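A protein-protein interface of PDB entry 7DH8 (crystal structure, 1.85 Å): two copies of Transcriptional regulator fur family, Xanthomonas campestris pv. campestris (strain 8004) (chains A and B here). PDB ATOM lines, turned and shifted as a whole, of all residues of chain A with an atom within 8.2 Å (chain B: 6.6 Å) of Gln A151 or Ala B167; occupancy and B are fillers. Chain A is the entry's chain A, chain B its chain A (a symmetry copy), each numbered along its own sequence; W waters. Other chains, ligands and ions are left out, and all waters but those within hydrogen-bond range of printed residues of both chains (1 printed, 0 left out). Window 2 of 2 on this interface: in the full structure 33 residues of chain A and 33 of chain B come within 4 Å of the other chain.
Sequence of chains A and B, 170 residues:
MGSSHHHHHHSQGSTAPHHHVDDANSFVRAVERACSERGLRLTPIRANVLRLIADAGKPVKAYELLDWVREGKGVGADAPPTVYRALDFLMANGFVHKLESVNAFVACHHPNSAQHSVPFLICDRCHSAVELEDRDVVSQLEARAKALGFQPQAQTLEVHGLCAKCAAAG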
ATOM      1  N   GLU A 142      23.125 -26.034  -9.210  1.00  0.00           N
ATOM      2  CA  GLU A 142      22.197 -25.236  -8.414  1.00  0.00           C
ATOM      3  C   GLU A 142      20.745 -25.511  -8.783  1.00  0.00           C
ATOM      4  O   GLU A 142      19.895 -25.703  -7.896  1.00  0.00           O
ATOM      5  CB  GLU A 142      22.496 -23.755  -8.547  1.00  0.00           C
ATOM      6  CG  GLU A 142      23.598 -23.290  -7.651  1.00  0.00           C
ATOM      7  CD  GLU A 142      23.871 -21.831  -7.900  1.00  0.00           C
ATOM      8  OE1 GLU A 142      22.925 -21.145  -8.349  1.00  0.00           O
ATOM      9  OE2 GLU A 142      25.006 -21.376  -7.652  1.00  0.00           O
ATOM     10  N   ALA A 145      19.583 -28.768  -7.432  1.00  0.00           N
ATOM     11  CA  ALA A 145      19.343 -28.664  -5.995  1.00  0.00           C
ATOM     12  C   ALA A 145      18.029 -27.957  -5.706  1.00  0.00           C
ATOM     13  O   ALA A 145      17.211 -28.448  -4.927  1.00  0.00           O
ATOM     14  CB  ALA A 145      20.518 -27.938  -5.317  1.00  0.00           C
ATOM     15  N   LYS A 146      17.785 -26.808  -6.366  1.00  0.00           N
ATOM     16  CA  LYS A 146      16.640 -26.010  -6.011  1.00  0.00           C
ATOM     17  C   LYS A 146      15.345 -26.683  -6.419  1.00  0.00           C
ATOM     18  O   LYS A 146      14.323 -26.465  -5.783  1.00  0.00           O
ATOM     19  CB  LYS A 146      16.749 -24.640  -6.635  1.00  0.00           C
ATOM     20  CG  LYS A 146      17.911 -23.873  -6.028  1.00  0.00           C
ATOM     21  CD  LYS A 146      17.835 -22.405  -6.427  1.00  0.00           C
ATOM     22  CE  LYS A 146      19.150 -21.723  -6.179  1.00  0.00           C
ATOM     23  NZ  LYS A 146      19.071 -20.329  -6.731  1.00  0.00           N
ATOM     24  N   ALA A 147      15.385 -27.534  -7.427  1.00  0.00           N
ATOM     25  CA  ALA A 147      14.179 -28.247  -7.866  1.00  0.00           C
ATOM     26  C   ALA A 147      13.774 -29.347  -6.898  1.00  0.00           C
ATOM     27  O   ALA A 147      12.650 -29.861  -7.001  1.00  0.00           O
ATOM     28  CB  ALA A 147      14.420 -28.857  -9.262  1.00  0.00           C
ATOM     29  N   LEU A 148      14.657 -29.723  -5.972  1.00  0.00           N
ATOM     30  CA  LEU A 148      14.298 -30.585  -4.848  1.00  0.00           C
ATOM     31  C   LEU A 148      14.163 -29.831  -3.543  1.00  0.00           C
ATOM     32  O   LEU A 148      14.181 -30.453  -2.472  1.00  0.00           O
ATOM     33  CB  LEU A 148      15.351 -31.685  -4.661  1.00  0.00           C
ATOM     34  CG  LEU A 148      15.562 -32.546  -5.891  1.00  0.00           C
ATOM     35  CD1 LEU A 148      16.863 -33.316  -5.765  1.00  0.00           C
ATOM     36  CD2 LEU A 148      14.339 -33.450  -6.011  1.00  0.00           C
ATOM     37  N   GLY A 149      14.077 -28.508  -3.579  1.00  0.00           N
ATOM     38  CA  GLY A 149      13.905 -27.798  -2.316  1.00  0.00           C
ATOM     39  C   GLY A 149      15.196 -27.547  -1.553  1.00  0.00           C
ATOM     40  O   GLY A 149      15.173 -26.849  -0.539  1.00  0.00           O
ATOM     41  N   PHE A 150      16.325 -28.070  -2.009  1.00  0.00           N
ATOM     42  CA  PHE A 150      17.604 -27.861  -1.330  1.00  0.00           C
ATOM     43  C   PHE A 150      18.139 -26.465  -1.657  1.00  0.00           C
ATOM     44  O   PHE A 150      18.122 -26.044  -2.811  1.00  0.00           O
ATOM     45  CB  PHE A 150      18.555 -28.965  -1.778  1.00  0.00           C
ATOM     46  CG  PHE A 150      19.881 -29.023  -1.033  1.00  0.00           C
ATOM     47  CD1 PHE A 150      20.977 -28.279  -1.468  1.00  0.00           C
ATOM     48  CD2 PHE A 150      20.030 -29.881   0.027  1.00  0.00           C
ATOM     49  CE1 PHE A 150      22.212 -28.389  -0.787  1.00  0.00           C
ATOM     50  CE2 PHE A 150      21.252 -29.982   0.698  1.00  0.00           C
ATOM     51  CZ  PHE A 150      22.331 -29.244   0.261  1.00  0.00           C
ATOM     52  N   GLN A 151      18.606 -25.733  -0.647  1.00  0.00           N
ATOM     53  CA  GLN A 151      19.087 -24.376  -0.906  1.00  0.00           C
ATOM     54  C   GLN A 151      20.635 -24.411  -0.999  1.00  0.00           C
ATOM     55  O   GLN A 151      21.324 -24.434   0.034  1.00  0.00           O
ATOM     56  CB  GLN A 151      18.598 -23.419   0.200  1.00  0.00           C
ATOM     57  CG  GLN A 151      17.022 -23.451   0.233  1.00  0.00           C
ATOM     58  CD  GLN A 151      16.341 -22.272   0.852  1.00  0.00           C
ATOM     59  OE1 GLN A 151      16.975 -21.318   1.291  1.00  0.00           O
ATOM     60  NE2 GLN A 151      14.993 -22.353   0.932  1.00  0.00           N
ATOM     61  N   PRO A 152      21.204 -24.429  -2.198  1.00  0.00           N
ATOM     62  CA  PRO A 152      22.644 -24.686  -2.354  1.00  0.00           C
ATOM     63  C   PRO A 152      23.684 -23.564  -2.348  1.00  0.00           C
ATOM     64  O   PRO A 152      23.667 -22.635  -3.170  1.00  0.00           O
ATOM     65  CB  PRO A 152      22.768 -25.090  -3.832  1.00  0.00           C
ATOM     66  CG  PRO A 152      21.629 -24.251  -4.514  1.00  0.00           C
ATOM     67  CD  PRO A 152      20.498 -24.168  -3.469  1.00  0.00           C
ATOM     68  N   GLN A 153      24.605 -23.678  -1.385  1.00  0.00           N
ATOM     69  CA  GLN A 153      25.716 -22.751  -1.270  1.00  0.00           C
ATOM     70  C   GLN A 153      27.196 -22.706  -1.658  1.00  0.00           C
ATOM     71  O   GLN A 153      27.687 -21.640  -2.054  1.00  0.00           O
ATOM     72  CB  GLN A 153      25.917 -22.589   0.248  1.00  0.00           C
ATOM     73  CG  GLN A 153      24.635 -22.137   0.954  1.00  0.00           C
ATOM     74  CD  GLN A 153      24.222 -20.713   0.596  1.00  0.00           C
ATOM     75  OE1 GLN A 153      24.969 -19.975  -0.080  1.00  0.00           O
ATOM     76  NE2 GLN A 153      23.037 -20.302   1.064  1.00  0.00           N
ATOM     77  N   ALA A 154      27.892 -23.830  -1.601  1.00  0.00           N
ATOM     78  CA  ALA A 154      29.297 -23.863  -2.009  1.00  0.00           C
ATOM     79  C   ALA A 154      29.233 -25.294  -2.557  1.00  0.00           C
ATOM     80  O   ALA A 154      28.652 -26.205  -1.952  1.00  0.00           O
ATOM     81  CB  ALA A 154      30.448 -23.962  -0.995  1.00  0.00           C
ATOM     82  N   CYS B 123      23.386 -31.729   3.309  1.00  0.00           N
ATOM     83  CA  CYS B 123      22.929 -30.599   4.088  1.00  0.00           C
ATOM     84  C   CYS B 123      24.018 -30.274   5.097  1.00  0.00           C
ATOM     85  O   CYS B 123      24.494 -31.165   5.794  1.00  0.00           O
ATOM     86  CB  CYS B 123      21.609 -30.913   4.802  1.00  0.00           C
ATOM     87  SG  CYS B 123      21.045 -29.583   5.841  1.00  0.00           S
ATOM     88  N   ARG B 125      23.575 -28.725   7.885  1.00  0.00           N
ATOM     89  CA  ARG B 125      23.117 -28.681   9.279  1.00  0.00           C
ATOM     90  C   ARG B 125      22.731 -30.072   9.810  1.00  0.00           C
ATOM     91  O   ARG B 125      23.194 -30.483  10.879  1.00  0.00           O
ATOM     92  CB  ARG B 125      21.956 -27.689   9.381  1.00  0.00           C
ATOM     93  CG  ARG B 125      21.313 -27.600  10.835  1.00  0.00           C
ATOM     94  CD  ARG B 125      20.440 -26.368  10.987  1.00  0.00           C
ATOM     95  NE  ARG B 125      21.101 -25.193  10.451  1.00  0.00           N
ATOM     96  CZ  ARG B 125      20.439 -24.208   9.863  1.00  0.00           C
ATOM     97  NH1 ARG B 125      19.115 -24.295   9.783  1.00  0.00           N
ATOM     98  NH2 ARG B 125      21.092 -23.156   9.357  1.00  0.00           N
ATOM     99  N   VAL B 159      27.260 -31.007  -3.405  1.00  0.00           N
ATOM    100  CA  VAL B 159      26.672 -29.678  -3.292  1.00  0.00           C
ATOM    101  C   VAL B 159      26.350 -29.444  -1.829  1.00  0.00           C
ATOM    102  O   VAL B 159      25.615 -30.243  -1.222  1.00  0.00           O
ATOM    103  CB  VAL B 159      25.434 -29.561  -4.193  1.00  0.00           C
ATOM    104  CG1 VAL B 159      24.776 -28.199  -4.019  1.00  0.00           C
ATOM    105  CG2 VAL B 159      25.858 -29.783  -5.655  1.00  0.00           C
ATOM    106  N   HIS B 160      26.838 -28.324  -1.277  1.00  0.00           N
ATOM    107  CA  HIS B 160      26.557 -27.967   0.110  1.00  0.00           C
ATOM    108  C   HIS B 160      25.491 -26.880   0.226  1.00  0.00           C
ATOM    109  O   HIS B 160      25.182 -26.156  -0.724  1.00  0.00           O
ATOM    110  CB  HIS B 160      27.823 -27.492   0.824  1.00  0.00           C
ATOM    111  CG  HIS B 160      29.004 -28.371   0.564  1.00  0.00           C
ATOM    112  ND1 HIS B 160      29.229 -29.552   1.257  1.00  0.00           N
ATOM    113  CD2 HIS B 160      30.038 -28.232  -0.312  1.00  0.00           C
ATOM    114  CE1 HIS B 160      30.352 -30.107   0.808  1.00  0.00           C
ATOM    115  NE2 HIS B 160      30.844 -29.337  -0.160  1.00  0.00           N
ATOM    116  N   GLY B 161      24.958 -26.757   1.430  1.00  0.00           N
ATOM    117  CA  GLY B 161      23.869 -25.826   1.701  1.00  0.00           C
ATOM    118  C   GLY B 161      22.922 -26.473   2.700  1.00  0.00           C
ATOM    119  O   GLY B 161      23.334 -27.318   3.537  1.00  0.00           O
ATOM    120  N   LEU B 162      21.633 -26.150   2.574  1.00  0.00           N
ATOM    121  CA  LEU B 162      20.622 -26.606   3.527  1.00  0.00           C
ATOM    122  C   LEU B 162      19.522 -27.378   2.811  1.00  0.00           C
ATOM    123  O   LEU B 162      18.995 -26.913   1.783  1.00  0.00           O
ATOM    124  CB  LEU B 162      19.996 -25.428   4.258  1.00  0.00           C
ATOM    125  CG  LEU B 162      20.973 -24.627   5.154  1.00  0.00           C
ATOM    126  CD1 LEU B 162      20.294 -23.368   5.744  1.00  0.00           C
ATOM    127  CD2 LEU B 162      21.628 -25.506   6.238  1.00  0.00           C
ATOM    128  N   CYS B 163      19.146 -28.525   3.376  1.00  0.00           N
ATOM    129  CA  CYS B 163      18.005 -29.226   2.806  1.00  0.00           C
ATOM    130  C   CYS B 163      16.706 -28.449   3.088  1.00  0.00           C
ATOM    131  O   CYS B 163      16.696 -27.454   3.820  1.00  0.00           O
ATOM    132  CB  CYS B 163      17.939 -30.639   3.348  1.00  0.00           C
ATOM    133  SG  CYS B 163      17.284 -30.627   5.146  1.00  0.00           S
ATOM    134  N   ALA B 164      15.611 -28.846   2.412  1.00  0.00           N
ATOM    135  CA  ALA B 164      14.359 -28.114   2.550  1.00  0.00           C
ATOM    136  C   ALA B 164      13.926 -28.008   4.000  1.00  0.00           C
ATOM    137  O   ALA B 164      13.449 -26.958   4.430  1.00  0.00           O
ATOM    138  CB  ALA B 164      13.232 -28.784   1.783  1.00  0.00           C
ATOM    139  N   LYS B 165      14.038 -29.097   4.756  1.00  0.00           N
ATOM    140  CA  LYS B 165      13.592 -29.061   6.167  1.00  0.00           C
ATOM    141  C   LYS B 165      14.363 -28.009   6.956  1.00  0.00           C
ATOM    142  O   LYS B 165      13.783 -27.197   7.683  1.00  0.00           O
ATOM    143  CB  LYS B 165      13.816 -30.425   6.832  1.00  0.00           C
ATOM    144  CG  LYS B 165      12.747 -31.422   6.635  1.00  0.00           C
ATOM    145  CD  LYS B 165      12.650 -32.020   5.239  1.00  0.00           C
ATOM    146  CE  LYS B 165      11.762 -33.265   5.321  1.00  0.00           C
ATOM    147  NZ  LYS B 165      12.430 -34.233   6.264  1.00  0.00           N
ATOM    148  N   CYS B 166      15.696 -28.014   6.825  1.00  0.00           N
ATOM    149  CA  CYS B 166      16.502 -27.082   7.596  1.00  0.00           C
ATOM    150  C   CYS B 166      16.335 -25.645   7.112  1.00  0.00           C
ATOM    151  O   CYS B 166      16.338 -24.719   7.933  1.00  0.00           O
ATOM    152  CB  CYS B 166      17.985 -27.488   7.565  1.00  0.00           C
ATOM    153  SG  CYS B 166      18.373 -29.074   8.435  1.00  0.00           S
ATOM    154  N   ALA B 167      16.203 -25.435   5.791  1.00  0.00           N
ATOM    155  CA  ALA B 167      15.972 -24.084   5.301  1.00  0.00           C
ATOM    156  C   ALA B 167      14.657 -23.518   5.809  1.00  0.00           C
ATOM    157  O   ALA B 167      14.525 -22.302   5.983  1.00  0.00           O
ATOM    158  CB  ALA B 167      15.988 -24.079   3.782  1.00  0.00           C
ATOM    159  N   ALA B 168      13.659 -24.374   6.026  1.00  0.00           N
ATOM    160  CA  ALA B 168      12.375 -23.895   6.506  1.00  0.00           C
ATOM    161  C   ALA B 168      12.377 -23.624   8.015  1.00  0.00           C
ATOM    162  O   ALA B 168      11.619 -22.788   8.467  1.00  0.00           O
ATOM    163  CB  ALA B 168      11.278 -24.895   6.148  1.00  0.00           C
ATOM    164  N   ALA B 169      13.231 -24.289   8.787  1.00  0.00           N
ATOM    165  CA  ALA B 169      13.401 -24.030  10.233  1.00  0.00           C
ATOM    166  C   ALA B 169      14.080 -22.683  10.442  1.00  0.00           C
ATOM    167  O   ALA B 169      15.086 -22.394   9.747  1.00  0.00           O
ATOM    168  CB  ALA B 169      14.249 -25.160  10.867  1.00  0.00           C
HETATM  169  O   HOH W   1      15.828 -30.869   0.346  1.00  0.00           O
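No position is printed for both chains.
Of the 16 pairs that touch across the chains among the printed residues, none has its exchanged pair printed and touching as well.
Of the 11 printed residues of chain A, 6 touch a printed residue of chain B.
Among the printed residues, no Asp or Glu carboxylate lies within 4 Å of a Lys or Arg side-chain nitrogen of the other chain.
Ala A147 touches none of the printed residues of chain B.
Printed residues of chain A within 4 Å of Cys B123: Phe A150.
Arg B125 touches none of the printed residues of chain A.
Of the printed residues of chain A, Val B159 touches Phe A150 (3.7 Å), Pro A152 (3.7 Å) and Ala A154 (3.98 Å).
Printed residues of chain A within 4 Å of His B160: Phe A150 (3.7 Å), Pro A152 (3.4 Å), Gln A153 (2.6 Å) and Ala A154 (2.9 Å).
Of the printed residues of chain A, Cys B163 touches Phe A150.
Of chain A, only Gln A151 comes within 4 Å of Ala B167.
No residue of chain A comes within 4 Å of Ala B168.
The backbone NH (N) of Gln A151 lies within hydrogen-bond range of the backbone carbonyl oxygen (O) of Leu B162 (2.7 Å).
The backbone NH of Gln A153 lies within hydrogen-bond range of the backbone carbonyl oxygen of His B160 (2.6 Å).
The backbone carbonyl oxygen (O) of Ala A154 lies within hydrogen-bond range of the backbone NH (N) of His B160, at 2.9 Å.
The backbone NH of Arg B125 sits close to the side-chain sulfur of Cys B123 (3.4 Å).
The backbone NH (N) of Phe A150 is in hydrogen-bond range of the backbone carbonyl oxygen (O) of Ala A145 (3.1 Å).
The side-chain sulfur of Cys B163 sits close to the backbone NH of Lys B165, at 3.6 Å.
Among the printed residues, pairs that only touch across the chains: Gly A149 with Ala B164 (3.4 Å), Phe A150 with Cys B123 (3.8 Å), Phe A150 with Val B159 (3.7 Å), Phe A150 with His B160 (3.7 Å), Phe A150 with Gly B161 (3.7 Å), Phe A150 with Leu B162 (3.5 Å), Phe A150 with Cys B163 (3.5 Å), Gln A151 with Gly B161 (3.3 Å), Gln A151 with Ala B167 (3.5 Å), Pro A152 with Val B159 (3.7 Å), Pro A152 with His B160 (3.4 Å), Gln A153 with Gly B161 (3.8 Å) and Ala A154 with Val B159 (3.98 Å).
Water W1 bridges the backbone NH of Ala B164 and the backbone carbonyl oxygen of Leu A148.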
